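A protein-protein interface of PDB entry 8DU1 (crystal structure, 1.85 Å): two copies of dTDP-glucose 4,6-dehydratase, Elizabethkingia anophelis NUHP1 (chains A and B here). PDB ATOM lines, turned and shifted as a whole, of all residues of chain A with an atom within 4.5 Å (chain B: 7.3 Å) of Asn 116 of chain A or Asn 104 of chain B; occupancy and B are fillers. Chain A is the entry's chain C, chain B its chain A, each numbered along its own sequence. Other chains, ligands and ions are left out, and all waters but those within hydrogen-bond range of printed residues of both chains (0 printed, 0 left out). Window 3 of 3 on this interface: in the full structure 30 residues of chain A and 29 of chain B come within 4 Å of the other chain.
The backbone carbonyl oxygen of Ile 69 of chain A sits at hydrogen-bond distance from the side-chain amide nitrogen of Asn 116 of chain A, at 2.8 Å.
O of Ile 112 of chain A lies close to ND2 of Asn 116 of chain A (3.5 Å).
The backbone carbonyl oxygen (O) of Ala 115 of chain A lies close to the side-chain amide nitrogen (ND2) of Asn 119 of chain A, at 3.2 Å.
The backbone carbonyl oxygen (O) of Asn 104 of chain B sits close to the side-chain amide nitrogen (ND2) of Asn 108 of chain B (3.5 Å).
Of chain A, only Ile 112, Ala 115, Asn 116 and Asn 119 come within 4 Å of Asn 104 of chain B.
Ala 115 of chain A touches just these residues of chain B: Asn 104 (3.7 Å) and Ile 107 (3.3 Å).
Printed residues of chain A within 4 Å of Ile 107 of chain B: Ile 112 and Ala 115.
Of the printed residues of chain A, Asn 108 of chain B touches Ile 112 (3.3 Å).
Of the printed residues of chain B, Ile 112 of chain A touches Asn 104 (3.7 Å), Ile 107 (3.5 Å) and Asn 108 (3.3 Å).
Of the printed residues of chain B, Asn 119 of chain A touches Asn 104.
The nearest residue of chain B that does not touch Asn 116 of chain A is Pro 103 of chain B (6.2 Å).
The nearest printed residue of chain A that does not touch Asn 104 of chain B is Pro 72 of chain A (5.9 Å).
The nearest printed residue of chain A that does not touch Ile 107 of chain B is Asn 116 of chain A (6.3 Å).
The side-chain amide oxygen (OD1) of Asn 116 of chain A is in hydrogen-bond range of the side-chain amide nitrogen (ND2) of Asn 104 of chain B.
The side-chain amide nitrogen (ND2) of Asn 119 of chain A lies within hydrogen-bond range of the side-chain amide oxygen (OD1) of Asn 104 of chain B.
Of the 14 printed residues of chain B, 3 touch a printed residue of chain A.
Printed residues of chain B that touch a printed residue of chain A: Asn 104, Ile 107 and Asn 108.
Hydrophobic or aromatic side chains of chain B within 4 Å of the printed part of chain A: Ile 107.
Among the printed residues, 7 pairs touch across the chains.
Among the printed residues, no Asp or Glu carboxylate lies within 4 Å of a Lys or Arg side-chain nitrogen of the other chain.
CD1 of Ile 112 of chain A touches CB of Asn 104 of chain B (3.7 Å).
Ile 107 of chain B touches Ile 112 of chain A.
Ile 112 of chain A touches Asn 108 of chain B (CD1 to OD1, 3.3 Å).
Asn 104 of chain B touches Ala 115 of chain A.
Ile 107 of chain B touches Ala 115 of chain A.
No position is printed for both chains.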
ATOM      1  N   ILE A  69      30.204 -13.200 -17.580  1.00  0.00           N
ATOM      2  CA  ILE A  69      29.528 -11.925 -17.361  1.00  0.00           C
ATOM      3  C   ILE A  69      28.138 -11.874 -17.970  1.00  0.00           C
ATOM      4  O   ILE A  69      27.382 -10.944 -17.673  1.00  0.00           O
ATOM      5  CB  ILE A  69      30.354 -10.732 -17.890  1.00  0.00           C
ATOM      6  CG1 ILE A  69      30.498 -10.781 -19.413  1.00  0.00           C
ATOM      7  CG2 ILE A  69      31.703 -10.707 -17.223  1.00  0.00           C
ATOM      8  CD1 ILE A  69      31.331  -9.616 -19.984  1.00  0.00           C
ATOM      9  N   THR A  70      27.778 -12.838 -18.819  1.00  0.00           N
ATOM     10  CA  THR A  70      26.394 -12.960 -19.258  1.00  0.00           C
ATOM     11  C   THR A  70      25.525 -13.728 -18.266  1.00  0.00           C
ATOM     12  O   THR A  70      24.338 -13.919 -18.540  1.00  0.00           O
ATOM     13  CB  THR A  70      26.315 -13.645 -20.627  1.00  0.00           C
ATOM     14  OG1 THR A  70      26.746 -15.009 -20.511  1.00  0.00           O
ATOM     15  CG2 THR A  70      27.190 -12.916 -21.650  1.00  0.00           C
ATOM     16  N   LYS A  71      26.077 -14.174 -17.134  1.00  0.00           N
ATOM     17  CA  LYS A  71      25.311 -14.900 -16.119  1.00  0.00           C
ATOM     18  C   LYS A  71      25.250 -14.071 -14.841  1.00  0.00           C
ATOM     19  O   LYS A  71      26.137 -14.184 -13.975  1.00  0.00           O
ATOM     20  CB  LYS A  71      25.931 -16.272 -15.846  1.00  0.00           C
ATOM     21  CG  LYS A  71      26.131 -17.118 -17.088  1.00  0.00           C
ATOM     22  CD  LYS A  71      24.826 -17.330 -17.835  1.00  0.00           C
ATOM     23  CE  LYS A  71      25.035 -18.253 -19.022  1.00  0.00           C
ATOM     24  NZ  LYS A  71      25.941 -19.381 -18.669  1.00  0.00           N
ATOM     25  N   PRO A  72      24.221 -13.233 -14.672  1.00  0.00           N
ATOM     26  CA  PRO A  72      24.153 -12.346 -13.496  1.00  0.00           C
ATOM     27  C   PRO A  72      24.341 -13.061 -12.172  1.00  0.00           C
ATOM     28  O   PRO A  72      24.925 -12.487 -11.241  1.00  0.00           O
ATOM     29  CB  PRO A  72      22.745 -11.737 -13.611  1.00  0.00           C
ATOM     30  CG  PRO A  72      22.464 -11.740 -15.082  1.00  0.00           C
ATOM     31  CD  PRO A  72      23.114 -12.994 -15.619  1.00  0.00           C
ATOM     32  N   LEU A  75      28.103 -13.597 -11.572  1.00  0.00           N
ATOM     33  CA  LEU A  75      28.715 -12.319 -11.226  1.00  0.00           C
ATOM     34  C   LEU A  75      28.347 -11.894  -9.812  1.00  0.00           C
ATOM     35  O   LEU A  75      29.194 -11.378  -9.072  1.00  0.00           O
ATOM     36  CB  LEU A  75      28.291 -11.243 -12.223  1.00  0.00           C
ATOM     37  CG  LEU A  75      28.873 -11.315 -13.624  1.00  0.00           C
ATOM     38  CD1 LEU A  75      28.362 -10.144 -14.446  1.00  0.00           C
ATOM     39  CD2 LEU A  75      30.406 -11.316 -13.555  1.00  0.00           C
ATOM     40  N   ILE A 112      25.339  -6.935 -23.215  1.00  0.00           N
ATOM     41  CA  ILE A 112      24.658  -7.375 -21.997  1.00  0.00           C
ATOM     42  C   ILE A 112      25.667  -7.661 -20.888  1.00  0.00           C
ATOM     43  O   ILE A 112      25.410  -7.398 -19.704  1.00  0.00           O
ATOM     44  CB  ILE A 112      23.775  -8.603 -22.294  1.00  0.00           C
ATOM     45  CG1 ILE A 112      22.515  -8.196 -23.077  1.00  0.00           C
ATOM     46  CG2 ILE A 112      23.362  -9.318 -21.005  1.00  0.00           C
ATOM     47  CD1 ILE A 112      21.396  -7.552 -22.219  1.00  0.00           C
ATOM     48  N   GLY A 113      26.814  -8.239 -21.242  1.00  0.00           N
ATOM     49  CA  GLY A 113      27.837  -8.469 -20.233  1.00  0.00           C
ATOM     50  C   GLY A 113      28.269  -7.183 -19.557  1.00  0.00           C
ATOM     51  O   GLY A 113      28.429  -7.134 -18.333  1.00  0.00           O
ATOM     52  N   THR A 114      28.447  -6.118 -20.343  1.00  0.00           N
ATOM     53  CA  THR A 114      28.836  -4.842 -19.759  1.00  0.00           C
ATOM     54  C   THR A 114      27.717  -4.282 -18.897  1.00  0.00           C
ATOM     55  O   THR A 114      27.968  -3.737 -17.821  1.00  0.00           O
ATOM     56  CB  THR A 114      29.228  -3.856 -20.866  1.00  0.00           C
ATOM     57  OG1 THR A 114      30.381  -4.354 -21.568  1.00  0.00           O
ATOM     58  CG2 THR A 114      29.562  -2.501 -20.273  1.00  0.00           C
ATOM     59  N   ALA A 115      26.468  -4.428 -19.338  1.00  0.00           N
ATOM     60  CA  ALA A 115      25.365  -3.947 -18.517  1.00  0.00           C
ATOM     61  C   ALA A 115      25.256  -4.734 -17.216  1.00  0.00           C
ATOM     62  O   ALA A 115      25.023  -4.150 -16.150  1.00  0.00           O
ATOM     63  CB  ALA A 115      24.055  -4.004 -19.308  1.00  0.00           C
ATOM     64  N   ASN A 116      25.443  -6.057 -17.270  1.00  0.00           N
ATOM     65  CA  ASN A 116      25.397  -6.856 -16.045  1.00  0.00           C
ATOM     66  C   ASN A 116      26.402  -6.362 -15.005  1.00  0.00           C
ATOM     67  O   ASN A 116      26.078  -6.254 -13.816  1.00  0.00           O
ATOM     68  CB  ASN A 116      25.650  -8.329 -16.372  1.00  0.00           C
ATOM     69  CG  ASN A 116      24.450  -8.987 -17.022  1.00  0.00           C
ATOM     70  OD1 ASN A 116      23.339  -8.470 -16.946  1.00  0.00           O
ATOM     71  ND2 ASN A 116      24.669 -10.129 -17.672  1.00  0.00           N
ATOM     72  N   LEU A 117      27.633  -6.069 -15.433  1.00  0.00           N
ATOM     73  CA  LEU A 117      28.642  -5.547 -14.513  1.00  0.00           C
ATOM     74  C   LEU A 117      28.267  -4.161 -13.996  1.00  0.00           C
ATOM     75  O   LEU A 117      28.440  -3.871 -12.806  1.00  0.00           O
ATOM     76  CB  LEU A 117      30.006  -5.507 -15.204  1.00  0.00           C
ATOM     77  CG  LEU A 117      30.607  -6.853 -15.607  1.00  0.00           C
ATOM     78  CD1 LEU A 117      31.682  -6.644 -16.658  1.00  0.00           C
ATOM     79  CD2 LEU A 117      31.192  -7.602 -14.387  1.00  0.00           C
ATOM     80  N   LEU A 118      27.767  -3.287 -14.882  1.00  0.00           N
ATOM     81  CA  LEU A 118      27.322  -1.956 -14.472  1.00  0.00           C
ATOM     82  C   LEU A 118      26.179  -2.034 -13.472  1.00  0.00           C
ATOM     83  O   LEU A 118      26.149  -1.289 -12.484  1.00  0.00           O
ATOM     84  CB  LEU A 118      26.883  -1.142 -15.698  1.00  0.00           C
ATOM     85  CG  LEU A 118      27.990  -0.725 -16.674  1.00  0.00           C
ATOM     86  CD1 LEU A 118      27.400  -0.157 -17.983  1.00  0.00           C
ATOM     87  CD2 LEU A 118      28.916   0.287 -16.019  1.00  0.00           C
ATOM     88  N   ASN A 119      25.211  -2.917 -13.719  1.00  0.00           N
ATOM     89  CA  ASN A 119      24.103  -3.063 -12.782  1.00  0.00           C
ATOM     90  C   ASN A 119      24.604  -3.472 -11.400  1.00  0.00           C
ATOM     91  O   ASN A 119      24.118  -2.970 -10.381  1.00  0.00           O
ATOM     92  CB  ASN A 119      23.103  -4.083 -13.314  1.00  0.00           C
ATOM     93  CG  ASN A 119      22.453  -3.640 -14.603  1.00  0.00           C
ATOM     94  OD1 ASN A 119      22.411  -2.451 -14.919  1.00  0.00           O
ATOM     95  ND2 ASN A 119      21.941  -4.601 -15.364  1.00  0.00           N
ATOM     96  N   LEU A 120      25.590  -4.369 -11.345  1.00  0.00           N
ATOM     97  CA  LEU A 120      26.091  -4.797 -10.042  1.00  0.00           C
ATOM     98  C   LEU A 120      26.919  -3.702  -9.388  1.00  0.00           C
ATOM     99  O   LEU A 120      26.862  -3.524  -8.167  1.00  0.00           O
ATOM    100  CB  LEU A 120      26.897  -6.083 -10.180  1.00  0.00           C
ATOM    101  CG  LEU A 120      26.001  -7.315 -10.288  1.00  0.00           C
ATOM    102  CD1 LEU A 120      26.777  -8.420 -10.955  1.00  0.00           C
ATOM    103  CD2 LEU A 120      25.516  -7.763  -8.907  1.00  0.00           C
ATOM    104  N   GLU B  93      11.884  -0.189 -26.377  1.00  0.00           N
ATOM    105  CA  GLU B  93      11.518  -0.175 -24.966  1.00  0.00           C
ATOM    106  C   GLU B  93      12.235   0.993 -24.314  1.00  0.00           C
ATOM    107  O   GLU B  93      13.457   1.082 -24.400  1.00  0.00           O
ATOM    108  CB  GLU B  93      11.929  -1.492 -24.300  1.00  0.00           C
ATOM    109  CG  GLU B  93      11.693  -1.536 -22.820  1.00  0.00           C
ATOM    110  CD  GLU B  93      10.237  -1.336 -22.501  1.00  0.00           C
ATOM    111  OE1 GLU B  93       9.434  -2.153 -22.980  1.00  0.00           O
ATOM    112  OE2 GLU B  93       9.913  -0.342 -21.807  1.00  0.00           O
ATOM    113  N   ASP B  97      14.451   0.613 -15.789  1.00  0.00           N
ATOM    114  CA  ASP B  97      14.116   0.425 -14.378  1.00  0.00           C
ATOM    115  C   ASP B  97      12.626   0.177 -14.150  1.00  0.00           C
ATOM    116  O   ASP B  97      12.132   0.354 -13.025  1.00  0.00           O
ATOM    117  CB  ASP B  97      14.613   1.604 -13.521  1.00  0.00           C
ATOM    118  CG  ASP B  97      16.139   1.666 -13.452  1.00  0.00           C
ATOM    119  OD1 ASP B  97      16.761   0.592 -13.294  1.00  0.00           O
ATOM    120  OD2 ASP B  97      16.718   2.773 -13.574  1.00  0.00           O
ATOM    121  N   SER B  99      11.152  -2.782 -14.026  1.00  0.00           N
ATOM    122  CA  SER B  99      10.973  -3.918 -13.128  1.00  0.00           C
ATOM    123  C   SER B  99      12.308  -4.596 -12.870  1.00  0.00           C
ATOM    124  O   SER B  99      13.053  -4.862 -13.814  1.00  0.00           O
ATOM    125  CB  SER B  99       9.985  -4.926 -13.727  1.00  0.00           C
ATOM    126  OG  SER B  99       9.830  -6.054 -12.886  1.00  0.00           O
ATOM    127  N   ILE B 100      12.597  -4.896 -11.600  1.00  0.00           N
ATOM    128  CA  ILE B 100      13.782  -5.683 -11.278  1.00  0.00           C
ATOM    129  C   ILE B 100      13.667  -7.114 -11.777  1.00  0.00           C
ATOM    130  O   ILE B 100      14.667  -7.843 -11.792  1.00  0.00           O
ATOM    131  CB  ILE B 100      14.055  -5.690  -9.762  1.00  0.00           C
ATOM    132  CG1 ILE B 100      12.914  -6.385  -9.013  1.00  0.00           C
ATOM    133  CG2 ILE B 100      14.235  -4.262  -9.247  1.00  0.00           C
ATOM    134  CD1 ILE B 100      13.223  -6.653  -7.542  1.00  0.00           C
ATOM    135  N   THR B 101      12.468  -7.545 -12.176  1.00  0.00           N
ATOM    136  CA  THR B 101      12.327  -8.863 -12.783  1.00  0.00           C
ATOM    137  C   THR B 101      12.966  -8.944 -14.169  1.00  0.00           C
ATOM    138  O   THR B 101      13.102 -10.053 -14.702  1.00  0.00           O
ATOM    139  CB  THR B 101      10.849  -9.244 -12.898  1.00  0.00           C
ATOM    140  OG1 THR B 101      10.232  -8.408 -13.881  1.00  0.00           O
ATOM    141  CG2 THR B 101      10.124  -9.092 -11.548  1.00  0.00           C
ATOM    142  N   ASP B 102      13.370  -7.814 -14.755  1.00  0.00           N
ATOM    143  CA  ASP B 102      13.937  -7.771 -16.101  1.00  0.00           C
ATOM    144  C   ASP B 102      14.760  -6.502 -16.284  1.00  0.00           C
ATOM    145  O   ASP B 102      14.391  -5.630 -17.076  1.00  0.00           O
ATOM    146  CB  ASP B 102      12.830  -7.836 -17.155  1.00  0.00           C
ATOM    147  CG  ASP B 102      13.335  -8.302 -18.522  1.00  0.00           C
ATOM    148  OD1 ASP B 102      14.566  -8.433 -18.713  1.00  0.00           O
ATOM    149  OD2 ASP B 102      12.490  -8.554 -19.403  1.00  0.00           O
ATOM    150  N   PRO B 103      15.893  -6.371 -15.590  1.00  0.00           N
ATOM    151  CA  PRO B 103      16.614  -5.083 -15.609  1.00  0.00           C
ATOM    152  C   PRO B 103      17.158  -4.699 -16.973  1.00  0.00           C
ATOM    153  O   PRO B 103      17.264  -3.505 -17.273  1.00  0.00           O
ATOM    154  CB  PRO B 103      17.749  -5.301 -14.595  1.00  0.00           C
ATOM    155  CG  PRO B 103      17.918  -6.792 -14.525  1.00  0.00           C
ATOM    156  CD  PRO B 103      16.540  -7.364 -14.715  1.00  0.00           C
ATOM    157  N   ASN B 104      17.520  -5.662 -17.818  1.00  0.00           N
ATOM    158  CA  ASN B 104      18.042  -5.325 -19.134  1.00  0.00           C
ATOM    159  C   ASN B 104      16.992  -5.454 -20.232  1.00  0.00           C
ATOM    160  O   ASN B 104      17.352  -5.647 -21.395  1.00  0.00           O
ATOM    161  CB  ASN B 104      19.263  -6.203 -19.458  1.00  0.00           C
ATOM    162  CG  ASN B 104      20.455  -5.900 -18.565  1.00  0.00           C
ATOM    163  OD1 ASN B 104      20.630  -4.771 -18.103  1.00  0.00           O
ATOM    164  ND2 ASN B 104      21.279  -6.913 -18.317  1.00  0.00           N
ATOM    165  N   ALA B 105      15.699  -5.348 -19.896  1.00  0.00           N
ATOM    166  CA  ALA B 105      14.679  -5.420 -20.941  1.00  0.00           C
ATOM    167  C   ALA B 105      14.952  -4.407 -22.047  1.00  0.00           C
ATOM    168  O   ALA B 105      14.806  -4.717 -23.235  1.00  0.00           O
ATOM    169  CB  ALA B 105      13.284  -5.211 -20.343  1.00  0.00           C
ATOM    170  N   PHE B 106      15.410  -3.206 -21.681  1.00  0.00           N
ATOM    171  CA  PHE B 106      15.647  -2.172 -22.682  1.00  0.00           C
ATOM    172  C   PHE B 106      16.734  -2.582 -23.662  1.00  0.00           C
ATOM    173  O   PHE B 106      16.629  -2.292 -24.855  1.00  0.00           O
ATOM    174  CB  PHE B 106      15.980  -0.826 -22.020  1.00  0.00           C
ATOM    175  CG  PHE B 106      17.329  -0.752 -21.381  1.00  0.00           C
ATOM    176  CD1 PHE B 106      17.572  -1.385 -20.175  1.00  0.00           C
ATOM    177  CD2 PHE B 106      18.344   0.011 -21.956  1.00  0.00           C
ATOM    178  CE1 PHE B 106      18.829  -1.289 -19.559  1.00  0.00           C
ATOM    179  CE2 PHE B 106      19.601   0.103 -21.353  1.00  0.00           C
ATOM    180  CZ  PHE B 106      19.838  -0.552 -20.146  1.00  0.00           C
ATOM    181  N   ILE B 107      17.781  -3.264 -23.187  1.00  0.00           N
ATOM    182  CA  ILE B 107      18.813  -3.746 -24.099  1.00  0.00           C
ATOM    183  C   ILE B 107      18.304  -4.927 -24.909  1.00  0.00           C
ATOM    184  O   ILE B 107      18.591  -5.046 -26.105  1.00  0.00           O
ATOM    185  CB  ILE B 107      20.081  -4.131 -23.316  1.00  0.00           C
ATOM    186  CG1 ILE B 107      20.635  -2.922 -22.575  1.00  0.00           C
ATOM    187  CG2 ILE B 107      21.127  -4.752 -24.273  1.00  0.00           C
ATOM    188  CD1 ILE B 107      21.726  -3.299 -21.591  1.00  0.00           C
ATOM    189  N   ASN B 108      17.574  -5.840 -24.265  1.00  0.00           N
ATOM    190  CA  ASN B 108      17.069  -7.013 -24.969  1.00  0.00           C
ATOM    191  C   ASN B 108      16.205  -6.597 -26.155  1.00  0.00           C
ATOM    192  O   ASN B 108      16.386  -7.082 -27.275  1.00  0.00           O
ATOM    193  CB  ASN B 108      16.283  -7.908 -23.998  1.00  0.00           C
ATOM    194  CG  ASN B 108      17.167  -8.540 -22.925  1.00  0.00           C
ATOM    195  OD1 ASN B 108      18.377  -8.663 -23.103  1.00  0.00           O
ATOM    196  ND2 ASN B 108      16.555  -8.979 -21.817  1.00  0.00           N
ATOM    197  N   THR B 109      15.258  -5.685 -25.926  1.00  0.00           N
ATOM    198  CA  THR B 109      14.407  -5.211 -27.014  1.00  0.00           C
ATOM    199  C   THR B 109      15.190  -4.348 -27.999  1.00  0.00           C
ATOM    200  O   THR B 109      15.119  -4.556 -29.218  1.00  0.00           O
ATOM    201  CB  THR B 109      13.229  -4.429 -26.437  1.00  0.00           C
ATOM    202  OG1 THR B 109      12.412  -5.325 -25.671  1.00  0.00           O
ATOM    203  CG2 THR B 109      12.395  -3.779 -27.567  1.00  0.00           C
ATOM    204  N   ASN B 110      15.927  -3.355 -27.493  1.00  0.00           N
ATOM    205  CA  ASN B 110      16.474  -2.337 -28.390  1.00  0.00           C
ATOM    206  C   ASN B 110      17.717  -2.808 -29.119  1.00  0.00           C
ATOM    207  O   ASN B 110      17.927  -2.421 -30.270  1.00  0.00           O
ATOM    208  CB  ASN B 110      16.780  -1.045 -27.629  1.00  0.00           C
ATOM    209  CG  ASN B 110      15.523  -0.451 -27.033  1.00  0.00           C
ATOM    210  OD1 ASN B 110      14.430  -0.912 -27.354  1.00  0.00           O
ATOM    211  ND2 ASN B 110      15.660   0.544 -26.173  1.00  0.00           N
